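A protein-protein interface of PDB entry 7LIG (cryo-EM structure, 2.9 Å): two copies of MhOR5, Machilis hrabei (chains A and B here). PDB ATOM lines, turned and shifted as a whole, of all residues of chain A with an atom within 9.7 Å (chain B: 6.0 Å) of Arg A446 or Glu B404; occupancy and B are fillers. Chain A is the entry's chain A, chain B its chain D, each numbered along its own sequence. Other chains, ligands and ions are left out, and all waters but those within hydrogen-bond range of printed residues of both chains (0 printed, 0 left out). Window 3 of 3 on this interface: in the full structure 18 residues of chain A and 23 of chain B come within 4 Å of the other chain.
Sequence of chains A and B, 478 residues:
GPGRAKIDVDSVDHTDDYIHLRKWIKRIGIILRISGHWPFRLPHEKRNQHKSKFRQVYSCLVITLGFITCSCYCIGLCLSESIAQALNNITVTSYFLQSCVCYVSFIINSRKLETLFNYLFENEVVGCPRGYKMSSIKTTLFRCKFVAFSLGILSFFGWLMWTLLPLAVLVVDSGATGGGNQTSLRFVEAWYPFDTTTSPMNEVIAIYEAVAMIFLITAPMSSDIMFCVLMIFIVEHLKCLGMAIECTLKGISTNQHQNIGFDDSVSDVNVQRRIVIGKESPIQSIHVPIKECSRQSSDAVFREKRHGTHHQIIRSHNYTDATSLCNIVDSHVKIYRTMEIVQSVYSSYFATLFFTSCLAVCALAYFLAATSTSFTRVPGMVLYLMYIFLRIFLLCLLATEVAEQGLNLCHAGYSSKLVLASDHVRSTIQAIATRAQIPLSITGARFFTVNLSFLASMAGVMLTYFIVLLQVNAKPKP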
ATOM      1  N   TYR A 336      16.895 -11.039   7.401  1.00  0.00           N
ATOM      2  CA  TYR A 336      16.547 -10.008   6.431  1.00  0.00           C
ATOM      3  C   TYR A 336      15.097 -10.124   5.984  1.00  0.00           C
ATOM      4  O   TYR A 336      14.413  -9.106   5.815  1.00  0.00           O
ATOM      5  CB  TYR A 336      17.477 -10.083   5.226  1.00  0.00           C
ATOM      6  CG  TYR A 336      17.018  -9.230   4.075  1.00  0.00           C
ATOM      7  CD1 TYR A 336      16.990  -7.850   4.185  1.00  0.00           C
ATOM      8  CD2 TYR A 336      16.608  -9.803   2.880  1.00  0.00           C
ATOM      9  CE1 TYR A 336      16.571  -7.060   3.135  1.00  0.00           C
ATOM     10  CE2 TYR A 336      16.187  -9.023   1.823  1.00  0.00           C
ATOM     11  CZ  TYR A 336      16.172  -7.652   1.958  1.00  0.00           C
ATOM     12  OH  TYR A 336      15.754  -6.866   0.911  1.00  0.00           O
ATOM     13  N   GLU A 340      12.203  -7.334   6.534  1.00  0.00           N
ATOM     14  CA  GLU A 340      11.402  -6.892   5.398  1.00  0.00           C
ATOM     15  C   GLU A 340       9.912  -7.040   5.680  1.00  0.00           C
ATOM     16  O   GLU A 340       9.105  -6.220   5.228  1.00  0.00           O
ATOM     17  CB  GLU A 340      11.800  -7.678   4.151  1.00  0.00           C
ATOM     18  CG  GLU A 340      11.125  -7.231   2.875  1.00  0.00           C
ATOM     19  CD  GLU A 340      11.654  -7.963   1.661  1.00  0.00           C
ATOM     20  OE1 GLU A 340      12.870  -7.874   1.395  1.00  0.00           O
ATOM     21  OE2 GLU A 340      10.857  -8.632   0.974  1.00  0.00           O
ATOM     22  N   GLN A 343       8.905  -4.186   8.075  1.00  0.00           N
ATOM     23  CA  GLN A 343       9.010  -2.850   7.484  1.00  0.00           C
ATOM     24  C   GLN A 343       7.656  -2.206   7.166  1.00  0.00           C
ATOM     25  O   GLN A 343       7.452  -1.025   7.450  1.00  0.00           O
ATOM     26  CB  GLN A 343       9.872  -2.924   6.223  1.00  0.00           C
ATOM     27  CG  GLN A 343       9.586  -1.864   5.172  1.00  0.00           C
ATOM     28  CD  GLN A 343       9.999  -0.477   5.610  1.00  0.00           C
ATOM     29  OE1 GLN A 343      10.890  -0.315   6.439  1.00  0.00           O
ATOM     30  NE2 GLN A 343       9.347   0.532   5.056  1.00  0.00           N
ATOM     31  N   SER A 344       6.699  -2.974   6.640  1.00  0.00           N
ATOM     32  CA  SER A 344       5.527  -2.372   5.994  1.00  0.00           C
ATOM     33  C   SER A 344       4.534  -1.780   6.998  1.00  0.00           C
ATOM     34  O   SER A 344       4.171  -0.586   6.922  1.00  0.00           O
ATOM     35  CB  SER A 344       4.836  -3.426   5.134  1.00  0.00           C
ATOM     36  OG  SER A 344       4.310  -4.454   5.951  1.00  0.00           O
ATOM     37  N   TYR A 346       4.764  -1.191  10.188  1.00  0.00           N
ATOM     38  CA  TYR A 346       5.314  -0.138  11.008  1.00  0.00           C
ATOM     39  C   TYR A 346       5.775   1.039  10.169  1.00  0.00           C
ATOM     40  O   TYR A 346       5.943   2.121  10.711  1.00  0.00           O
ATOM     41  CB  TYR A 346       6.431  -0.693  11.874  1.00  0.00           C
ATOM     42  CG  TYR A 346       5.885  -1.579  12.959  1.00  0.00           C
ATOM     43  CD1 TYR A 346       5.855  -2.952  12.809  1.00  0.00           C
ATOM     44  CD2 TYR A 346       5.366  -1.036  14.118  1.00  0.00           C
ATOM     45  CE1 TYR A 346       5.344  -3.761  13.792  1.00  0.00           C
ATOM     46  CE2 TYR A 346       4.853  -1.834  15.105  1.00  0.00           C
ATOM     47  CZ  TYR A 346       4.848  -3.195  14.938  1.00  0.00           C
ATOM     48  OH  TYR A 346       4.336  -3.993  15.926  1.00  0.00           O
ATOM     49  N   SER A 347       5.887   0.889   8.847  1.00  0.00           N
ATOM     50  CA  SER A 347       6.150   2.056   8.013  1.00  0.00           C
ATOM     51  C   SER A 347       4.964   3.005   8.026  1.00  0.00           C
ATOM     52  O   SER A 347       5.109   4.203   8.325  1.00  0.00           O
ATOM     53  CB  SER A 347       6.471   1.620   6.586  1.00  0.00           C
ATOM     54  OG  SER A 347       5.355   1.828   5.740  1.00  0.00           O
ATOM     55  N   SER A 348       3.773   2.467   7.746  1.00  0.00           N
ATOM     56  CA  SER A 348       2.573   3.308   7.788  1.00  0.00           C
ATOM     57  C   SER A 348       2.315   3.846   9.195  1.00  0.00           C
ATOM     58  O   SER A 348       2.072   5.059   9.383  1.00  0.00           O
ATOM     59  CB  SER A 348       1.366   2.526   7.284  1.00  0.00           C
ATOM     60  OG  SER A 348       1.522   2.200   5.916  1.00  0.00           O
ATOM     61  N   TYR A 349       2.428   2.968  10.199  1.00  0.00           N
ATOM     62  CA  TYR A 349       2.160   3.372  11.572  1.00  0.00           C
ATOM     63  C   TYR A 349       3.175   4.396  12.072  1.00  0.00           C
ATOM     64  O   TYR A 349       2.810   5.326  12.796  1.00  0.00           O
ATOM     65  CB  TYR A 349       2.142   2.141  12.469  1.00  0.00           C
ATOM     66  CG  TYR A 349       2.116   2.448  13.936  1.00  0.00           C
ATOM     67  CD1 TYR A 349       3.232   2.231  14.724  1.00  0.00           C
ATOM     68  CD2 TYR A 349       0.973   2.941  14.539  1.00  0.00           C
ATOM     69  CE1 TYR A 349       3.213   2.503  16.062  1.00  0.00           C
ATOM     70  CE2 TYR A 349       0.945   3.216  15.881  1.00  0.00           C
ATOM     71  CZ  TYR A 349       2.068   2.994  16.641  1.00  0.00           C
ATOM     72  OH  TYR A 349       2.047   3.270  17.987  1.00  0.00           O
ATOM     73  N   PHE A 350       4.440   4.280  11.654  1.00  0.00           N
ATOM     74  CA  PHE A 350       5.465   5.195  12.136  1.00  0.00           C
ATOM     75  C   PHE A 350       5.337   6.556  11.485  1.00  0.00           C
ATOM     76  O   PHE A 350       5.611   7.570  12.133  1.00  0.00           O
ATOM     77  CB  PHE A 350       6.863   4.634  11.883  1.00  0.00           C
ATOM     78  CG  PHE A 350       7.293   3.594  12.871  1.00  0.00           C
ATOM     79  CD1 PHE A 350       6.536   3.318  13.989  1.00  0.00           C
ATOM     80  CD2 PHE A 350       8.442   2.862  12.648  1.00  0.00           C
ATOM     81  CE1 PHE A 350       6.926   2.347  14.876  1.00  0.00           C
ATOM     82  CE2 PHE A 350       8.839   1.893  13.533  1.00  0.00           C
ATOM     83  CZ  PHE A 350       8.082   1.635  14.649  1.00  0.00           C
ATOM     84  N   ALA A 351       4.933   6.604  10.209  1.00  0.00           N
ATOM     85  CA  ALA A 351       4.691   7.900   9.576  1.00  0.00           C
ATOM     86  C   ALA A 351       3.602   8.673  10.313  1.00  0.00           C
ATOM     87  O   ALA A 351       3.813   9.833  10.724  1.00  0.00           O
ATOM     88  CB  ALA A 351       4.316   7.707   8.110  1.00  0.00           C
ATOM     89  N   THR A 352       2.455   8.012  10.548  1.00  0.00           N
ATOM     90  CA  THR A 352       1.366   8.659  11.286  1.00  0.00           C
ATOM     91  C   THR A 352       1.798   9.051  12.696  1.00  0.00           C
ATOM     92  O   THR A 352       1.553  10.186  13.141  1.00  0.00           O
ATOM     93  CB  THR A 352       0.152   7.732  11.343  1.00  0.00           C
ATOM     94  OG1 THR A 352      -0.401   7.587  10.032  1.00  0.00           O
ATOM     95  CG2 THR A 352      -0.915   8.290  12.263  1.00  0.00           C
ATOM     96  N   ILE A 438      24.611  -3.643   3.301  1.00  0.00           N
ATOM     97  CA  ILE A 438      23.307  -2.986   3.168  1.00  0.00           C
ATOM     98  C   ILE A 438      22.640  -2.928   4.533  1.00  0.00           C
ATOM     99  O   ILE A 438      22.449  -3.983   5.172  1.00  0.00           O
ATOM    100  CB  ILE A 438      22.428  -3.732   2.156  1.00  0.00           C
ATOM    101  CG1 ILE A 438      23.074  -3.704   0.774  1.00  0.00           C
ATOM    102  CG2 ILE A 438      21.049  -3.115   2.101  1.00  0.00           C
ATOM    103  CD1 ILE A 438      23.439  -2.321   0.306  1.00  0.00           C
ATOM    104  N   SER A 441      17.130  -1.179   7.907  1.00  0.00           N
ATOM    105  CA  SER A 441      16.559   0.061   8.409  1.00  0.00           C
ATOM    106  C   SER A 441      15.045   0.002   8.317  1.00  0.00           C
ATOM    107  O   SER A 441      14.500  -0.505   7.333  1.00  0.00           O
ATOM    108  CB  SER A 441      17.085   1.255   7.619  1.00  0.00           C
ATOM    109  OG  SER A 441      17.053   0.984   6.230  1.00  0.00           O
ATOM    110  N   ILE A 442      14.372   0.523   9.335  1.00  0.00           N
ATOM    111  CA  ILE A 442      12.923   0.654   9.320  1.00  0.00           C
ATOM    112  C   ILE A 442      12.591   2.088   8.941  1.00  0.00           C
ATOM    113  O   ILE A 442      12.920   3.024   9.675  1.00  0.00           O
ATOM    114  CB  ILE A 442      12.315   0.289  10.678  1.00  0.00           C
ATOM    115  CG1 ILE A 442      12.465  -1.205  10.931  1.00  0.00           C
ATOM    116  CG2 ILE A 442      10.854   0.664  10.717  1.00  0.00           C
ATOM    117  CD1 ILE A 442      11.762  -2.052   9.914  1.00  0.00           C
ATOM    118  N   THR A 443      11.950   2.264   7.796  1.00  0.00           N
ATOM    119  CA  THR A 443      11.604   3.584   7.294  1.00  0.00           C
ATOM    120  C   THR A 443      10.131   3.852   7.542  1.00  0.00           C
ATOM    121  O   THR A 443       9.311   2.934   7.512  1.00  0.00           O
ATOM    122  CB  THR A 443      11.903   3.696   5.802  1.00  0.00           C
ATOM    123  OG1 THR A 443      11.142   2.712   5.092  1.00  0.00           O
ATOM    124  CG2 THR A 443      13.377   3.472   5.537  1.00  0.00           C
ATOM    125  N   GLY A 444       9.800   5.112   7.792  1.00  0.00           N
ATOM    126  CA  GLY A 444       8.410   5.469   7.988  1.00  0.00           C
ATOM    127  C   GLY A 444       7.739   5.885   6.699  1.00  0.00           C
ATOM    128  O   GLY A 444       7.834   7.048   6.300  1.00  0.00           O
ATOM    129  N   ALA A 445       7.051   4.936   6.054  1.00  0.00           N
ATOM    130  CA  ALA A 445       6.417   5.094   4.742  1.00  0.00           C
ATOM    131  C   ALA A 445       7.369   5.641   3.688  1.00  0.00           C
ATOM    132  O   ALA A 445       6.946   6.405   2.817  1.00  0.00           O
ATOM    133  CB  ALA A 445       5.167   5.974   4.822  1.00  0.00           C
ATOM    134  N   ARG A 446       8.652   5.284   3.788  1.00  0.00           N
ATOM    135  CA  ARG A 446       9.763   5.703   2.934  1.00  0.00           C
ATOM    136  C   ARG A 446      10.035   7.201   2.965  1.00  0.00           C
ATOM    137  O   ARG A 446      10.827   7.687   2.154  1.00  0.00           O
ATOM    138  CB  ARG A 446       9.568   5.253   1.484  1.00  0.00           C
ATOM    139  CG  ARG A 446       9.335   3.771   1.345  1.00  0.00           C
ATOM    140  CD  ARG A 446       9.534   3.335  -0.081  1.00  0.00           C
ATOM    141  NE  ARG A 446       8.285   3.358  -0.828  1.00  0.00           N
ATOM    142  CZ  ARG A 446       7.473   2.316  -0.940  1.00  0.00           C
ATOM    143  NH1 ARG A 446       7.785   1.171  -0.351  1.00  0.00           N
ATOM    144  NH2 ARG A 446       6.353   2.415  -1.640  1.00  0.00           N
ATOM    145  N   PHE A 447       9.419   7.951   3.879  1.00  0.00           N
ATOM    146  CA  PHE A 447       9.693   9.377   3.986  1.00  0.00           C
ATOM    147  C   PHE A 447      10.960   9.669   4.770  1.00  0.00           C
ATOM    148  O   PHE A 447      11.669  10.626   4.443  1.00  0.00           O
ATOM    149  CB  PHE A 447       8.524  10.098   4.654  1.00  0.00           C
ATOM    150  CG  PHE A 447       7.330  10.264   3.773  1.00  0.00           C
ATOM    151  CD1 PHE A 447       7.337  11.183   2.746  1.00  0.00           C
ATOM    152  CD2 PHE A 447       6.193   9.508   3.981  1.00  0.00           C
ATOM    153  CE1 PHE A 447       6.236  11.340   1.936  1.00  0.00           C
ATOM    154  CE2 PHE A 447       5.089   9.662   3.175  1.00  0.00           C
ATOM    155  CZ  PHE A 447       5.112  10.579   2.151  1.00  0.00           C
ATOM    156  N   PHE A 448      11.255   8.878   5.795  1.00  0.00           N
ATOM    157  CA  PHE A 448      12.432   9.097   6.619  1.00  0.00           C
ATOM    158  C   PHE A 448      12.879   7.761   7.187  1.00  0.00           C
ATOM    159  O   PHE A 448      12.123   6.787   7.213  1.00  0.00           O
ATOM    160  CB  PHE A 448      12.154  10.103   7.739  1.00  0.00           C
ATOM    161  CG  PHE A 448      10.812   9.931   8.393  1.00  0.00           C
ATOM    162  CD1 PHE A 448      10.605   8.944   9.339  1.00  0.00           C
ATOM    163  CD2 PHE A 448       9.763  10.770   8.073  1.00  0.00           C
ATOM    164  CE1 PHE A 448       9.379   8.790   9.938  1.00  0.00           C
ATOM    165  CE2 PHE A 448       8.534  10.622   8.675  1.00  0.00           C
ATOM    166  CZ  PHE A 448       8.344   9.628   9.607  1.00  0.00           C
ATOM    167  N   THR A 449      14.121   7.731   7.650  1.00  0.00           N
ATOM    168  CA  THR A 449      14.698   6.555   8.277  1.00  0.00           C
ATOM    169  C   THR A 449      14.654   6.725   9.786  1.00  0.00           C
ATOM    170  O   THR A 449      15.176   7.710  10.314  1.00  0.00           O
ATOM    171  CB  THR A 449      16.138   6.351   7.814  1.00  0.00           C
ATOM    172  OG1 THR A 449      16.253   6.743   6.442  1.00  0.00           O
ATOM    173  CG2 THR A 449      16.537   4.903   7.953  1.00  0.00           C
ATOM    174  N   VAL A 450      14.038   5.769  10.476  1.00  0.00           N
ATOM    175  CA  VAL A 450      13.913   5.861  11.924  1.00  0.00           C
ATOM    176  C   VAL A 450      15.271   5.573  12.542  1.00  0.00           C
ATOM    177  O   VAL A 450      15.673   4.415  12.690  1.00  0.00           O
ATOM    178  CB  VAL A 450      12.840   4.904  12.462  1.00  0.00           C
ATOM    179  CG1 VAL A 450      12.710   5.054  13.956  1.00  0.00           C
ATOM    180  CG2 VAL A 450      11.517   5.187  11.802  1.00  0.00           C
ATOM    181  N   PHE A 454      17.378  11.166  13.410  1.00  0.00           N
ATOM    182  CA  PHE A 454      16.052  11.670  13.084  1.00  0.00           C
ATOM    183  C   PHE A 454      15.369  12.257  14.305  1.00  0.00           C
ATOM    184  O   PHE A 454      14.606  13.220  14.184  1.00  0.00           O
ATOM    185  CB  PHE A 454      15.194  10.562  12.490  1.00  0.00           C
ATOM    186  CG  PHE A 454      13.819  11.007  12.137  1.00  0.00           C
ATOM    187  CD1 PHE A 454      13.615  11.862  11.076  1.00  0.00           C
ATOM    188  CD2 PHE A 454      12.732  10.590  12.877  1.00  0.00           C
ATOM    189  CE1 PHE A 454      12.352  12.284  10.748  1.00  0.00           C
ATOM    190  CE2 PHE A 454      11.465  11.008  12.555  1.00  0.00           C
ATOM    191  CZ  PHE A 454      11.274  11.856  11.488  1.00  0.00           C
ATOM    192  N   LEU B 397       6.608   8.908  -5.678  1.00  0.00           N
ATOM    193  CA  LEU B 397       6.381   7.510  -5.329  1.00  0.00           C
ATOM    194  C   LEU B 397       6.933   6.577  -6.397  1.00  0.00           C
ATOM    195  O   LEU B 397       7.649   5.612  -6.093  1.00  0.00           O
ATOM    196  CB  LEU B 397       4.891   7.262  -5.124  1.00  0.00           C
ATOM    197  CG  LEU B 397       4.535   5.828  -4.765  1.00  0.00           C
ATOM    198  CD1 LEU B 397       5.117   5.501  -3.415  1.00  0.00           C
ATOM    199  CD2 LEU B 397       3.036   5.643  -4.755  1.00  0.00           C
ATOM    200  N   ALA B 399       9.209   7.279  -8.465  1.00  0.00           N
ATOM    201  CA  ALA B 399      10.662   7.362  -8.525  1.00  0.00           C
ATOM    202  C   ALA B 399      11.323   6.643  -7.359  1.00  0.00           C
ATOM    203  O   ALA B 399      12.482   6.233  -7.473  1.00  0.00           O
ATOM    204  CB  ALA B 399      11.111   8.821  -8.559  1.00  0.00           C
ATOM    205  N   THR B 400      10.618   6.486  -6.234  1.00  0.00           N
ATOM    206  CA  THR B 400      11.197   5.761  -5.106  1.00  0.00           C
ATOM    207  C   THR B 400      11.093   4.253  -5.300  1.00  0.00           C
ATOM    208  O   THR B 400      11.960   3.494  -4.831  1.00  0.00           O
ATOM    209  CB  THR B 400      10.506   6.178  -3.811  1.00  0.00           C
ATOM    210  OG1 THR B 400      10.346   7.599  -3.798  1.00  0.00           O
ATOM    211  CG2 THR B 400      11.332   5.774  -2.605  1.00  0.00           C
ATOM    212  N   GLU B 401      10.037   3.806  -5.990  1.00  0.00           N
ATOM    213  CA  GLU B 401       9.818   2.373  -6.179  1.00  0.00           C
ATOM    214  C   GLU B 401      10.941   1.726  -6.980  1.00  0.00           C
ATOM    215  O   GLU B 401      11.321   0.582  -6.709  1.00  0.00           O
ATOM    216  CB  GLU B 401       8.479   2.136  -6.869  1.00  0.00           C
ATOM    217  CG  GLU B 401       7.307   2.097  -5.925  1.00  0.00           C
ATOM    218  CD  GLU B 401       7.395   0.949  -4.951  1.00  0.00           C
ATOM    219  OE1 GLU B 401       7.044  -0.184  -5.336  1.00  0.00           O
ATOM    220  OE2 GLU B 401       7.811   1.178  -3.798  1.00  0.00           O
ATOM    221  N   VAL B 402      11.504   2.453  -7.945  1.00  0.00           N
ATOM    222  CA  VAL B 402      12.550   1.888  -8.793  1.00  0.00           C
ATOM    223  C   VAL B 402      13.829   1.668  -7.995  1.00  0.00           C
ATOM    224  O   VAL B 402      14.476   0.616  -8.107  1.00  0.00           O
ATOM    225  CB  VAL B 402      12.769   2.800 -10.013  1.00  0.00           C
ATOM    226  CG1 VAL B 402      14.183   2.699 -10.546  1.00  0.00           C
ATOM    227  CG2 VAL B 402      11.785   2.452 -11.085  1.00  0.00           C
ATOM    228  N   ALA B 403      14.196   2.637  -7.154  1.00  0.00           N
ATOM    229  CA  ALA B 403      15.378   2.487  -6.314  1.00  0.00           C
ATOM    230  C   ALA B 403      15.196   1.369  -5.298  1.00  0.00           C
ATOM    231  O   ALA B 403      16.137   0.608  -5.025  1.00  0.00           O
ATOM    232  CB  ALA B 403      15.691   3.804  -5.608  1.00  0.00           C
ATOM    233  N   GLU B 404      13.983   1.236  -4.748  1.00  0.00           N
ATOM    234  CA  GLU B 404      13.741   0.143  -3.811  1.00  0.00           C
ATOM    235  C   GLU B 404      13.807  -1.213  -4.500  1.00  0.00           C
ATOM    236  O   GLU B 404      14.307  -2.182  -3.920  1.00  0.00           O
ATOM    237  CB  GLU B 404      12.397   0.316  -3.115  1.00  0.00           C
ATOM    238  CG  GLU B 404      12.368  -0.320  -1.740  1.00  0.00           C
ATOM    239  CD  GLU B 404      11.561   0.475  -0.744  1.00  0.00           C
ATOM    240  OE1 GLU B 404      10.349   0.205  -0.622  1.00  0.00           O
ATOM    241  OE2 GLU B 404      12.138   1.359  -0.076  1.00  0.00           O
ATOM    242  N   GLN B 405      13.344  -1.300  -5.749  1.00  0.00           N
ATOM    243  CA  GLN B 405      13.445  -2.573  -6.454  1.00  0.00           C
ATOM    244  C   GLN B 405      14.880  -2.890  -6.851  1.00  0.00           C
ATOM    245  O   GLN B 405      15.258  -4.064  -6.890  1.00  0.00           O
ATOM    246  CB  GLN B 405      12.540  -2.584  -7.681  1.00  0.00           C
ATOM    247  CG  GLN B 405      11.065  -2.630  -7.350  1.00  0.00           C
ATOM    248  CD  GLN B 405      10.749  -3.575  -6.215  1.00  0.00           C
ATOM    249  OE1 GLN B 405      11.039  -4.767  -6.282  1.00  0.00           O
ATOM    250  NE2 GLN B 405      10.143  -3.045  -5.163  1.00  0.00           N
ATOM    251  N   GLY B 406      15.697  -1.872  -7.121  1.00  0.00           N
ATOM    252  CA  GLY B 406      17.111  -2.128  -7.368  1.00  0.00           C
ATOM    253  C   GLY B 406      17.826  -2.657  -6.138  1.00  0.00           C
ATOM    254  O   GLY B 406      18.581  -3.638  -6.204  1.00  0.00           O
ATOM    255  N   LEU B 407      17.574  -2.031  -4.987  1.00  0.00           N
ATOM    256  CA  LEU B 407      18.193  -2.501  -3.749  1.00  0.00           C
ATOM    257  C   LEU B 407      17.647  -3.864  -3.337  1.00  0.00           C
ATOM    258  O   LEU B 407      18.338  -4.645  -2.673  1.00  0.00           O
ATOM    259  CB  LEU B 407      17.994  -1.477  -2.634  1.00  0.00           C
ATOM    260  CG  LEU B 407      19.129  -0.481  -2.390  1.00  0.00           C
ATOM    261  CD1 LEU B 407      20.392  -1.222  -2.008  1.00  0.00           C
ATOM    262  CD2 LEU B 407      19.378   0.412  -3.592  1.00  0.00           C
ATOM    263  N   ASN B 408      16.406  -4.174  -3.722  1.00  0.00           N
ATOM    264  CA  ASN B 408      15.887  -5.518  -3.491  1.00  0.00           C
ATOM    265  C   ASN B 408      16.526  -6.528  -4.431  1.00  0.00           C
ATOM    266  O   ASN B 408      16.685  -7.697  -4.067  1.00  0.00           O
ATOM    267  CB  ASN B 408      14.371  -5.537  -3.653  1.00  0.00           C
ATOM    268  CG  ASN B 408      13.650  -5.097  -2.402  1.00  0.00           C
ATOM    269  OD1 ASN B 408      14.251  -4.514  -1.501  1.00  0.00           O
ATOM    270  ND2 ASN B 408      12.355  -5.374  -2.337  1.00  0.00           N
ATOM    271  N   LEU B 409      16.880  -6.102  -5.645  1.00  0.00           N
ATOM    272  CA  LEU B 409      17.649  -6.942  -6.554  1.00  0.00           C
ATOM    273  C   LEU B 409      19.044  -7.233  -6.026  1.00  0.00           C
ATOM    274  O   LEU B 409      19.600  -8.288  -6.350  1.00  0.00           O
ATOM    275  CB  LEU B 409      17.741  -6.282  -7.931  1.00  0.00           C
ATOM    276  CG  LEU B 409      18.371  -7.083  -9.068  1.00  0.00           C
ATOM    277  CD1 LEU B 409      17.553  -8.324  -9.344  1.00  0.00           C
ATOM    278  CD2 LEU B 409      18.510  -6.237 -10.314  1.00  0.00           C
ATOM    279  N   LEU B 452      10.977  10.237  -1.911  1.00  0.00           N
ATOM    280  CA  LEU B 452       9.876  10.648  -1.056  1.00  0.00           C
ATOM    281  C   LEU B 452      10.340  11.529   0.092  1.00  0.00           C
ATOM    282  O   LEU B 452       9.543  12.320   0.605  1.00  0.00           O
ATOM    283  CB  LEU B 452       9.137   9.425  -0.521  1.00  0.00           C
ATOM    284  CG  LEU B 452       8.076   8.882  -1.473  1.00  0.00           C
ATOM    285  CD1 LEU B 452       7.495   7.588  -0.952  1.00  0.00           C
ATOM    286  CD2 LEU B 452       6.989   9.912  -1.646  1.00  0.00           C
ATOM    287  N   SER B 453      11.605  11.421   0.499  1.00  0.00           N
ATOM    288  CA  SER B 453      12.139  12.325   1.510  1.00  0.00           C
ATOM    289  C   SER B 453      12.273  13.742   0.978  1.00  0.00           C
ATOM    290  O   SER B 453      12.151  14.711   1.743  1.00  0.00           O
ATOM    291  CB  SER B 453      13.496  11.825   1.998  1.00  0.00           C
ATOM    292  OG  SER B 453      14.532  12.322   1.174  1.00  0.00           O
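The side-chain carboxylate (OE2) of Glu B401 lies within salt-bridge range of the guanidinium group (NH2) of Arg A446, 2.9 Å away.
NH1 of Arg A446 is in salt-bridge range of OE1 of Glu B404, 2.8 Å away.
No position is printed for both chains.
Of the 10 pairs that touch across the chains among the printed residues, none has its exchanged pair printed and touching as well.
Tyr A336 touches Asn B408.
CD1 of Ile A438 touches CD1 of Leu B407, at 3.98 Å.
Ala A445 touches Leu B452 (O to CD1, 3.99 Å).
Leu B397 touches Arg A446.
CD of Arg A446 touches CG2 of Thr B400 (3.9 Å).
Arg A446 touches Leu B452 (O to CB, 3.6 Å).
Leu B452 touches Phe A447.
Phe A447 touches Ser B453.
OE1 of Glu A340 lies within hydrogen-bond range of OH of Tyr A336.
The backbone carbonyl oxygen (O) of Ser A347 lies within hydrogen-bond range of the backbone NH (N) of Ala A445.
The backbone NH of Leu B452 sits at hydrogen-bond distance from the side-chain hydroxyl of Thr B400, at 3.3 Å.
O of Glu B404 lies close to OD1 of Asn B408, at 3.4 Å.
Hydrophobic or aromatic side chains of chain B within 4 Å of the printed part of chain A: Leu B397, Leu B407 and Leu B452.
Of the 23 printed residues of chain A, 5 touch a printed residue of chain B.
Along chain A the printed residues that touch a printed residue of chain B span positions 336 to 447.
Among the printed residues, 10 pairs touch across the chains.
Among the printed residues, Asp or Glu carboxylates within 4 Å of a Lys or Arg side-chain nitrogen of the other chain: Arg A446 with Glu B401 (2.9 Å) and Arg A446 with Glu B404 (2.8 Å).
Of chain B, only Leu B397, Thr B400, Glu B401, Glu B404 and Leu B452 come within 4 Å of Arg A446.
No residue of chain A comes within 4 Å of Ala B403.
No residue of chain A comes within 4 Å of Gln B405.
Of the printed residues of chain B, Ile A438 touches Leu B407.
Of the printed residues of chain A, Glu B401 touches Arg A446.
Of the printed residues of chain B, Tyr A336 touches Asn B408 (3.7 Å).
Tyr A349 touches none of the printed residues of chain B.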
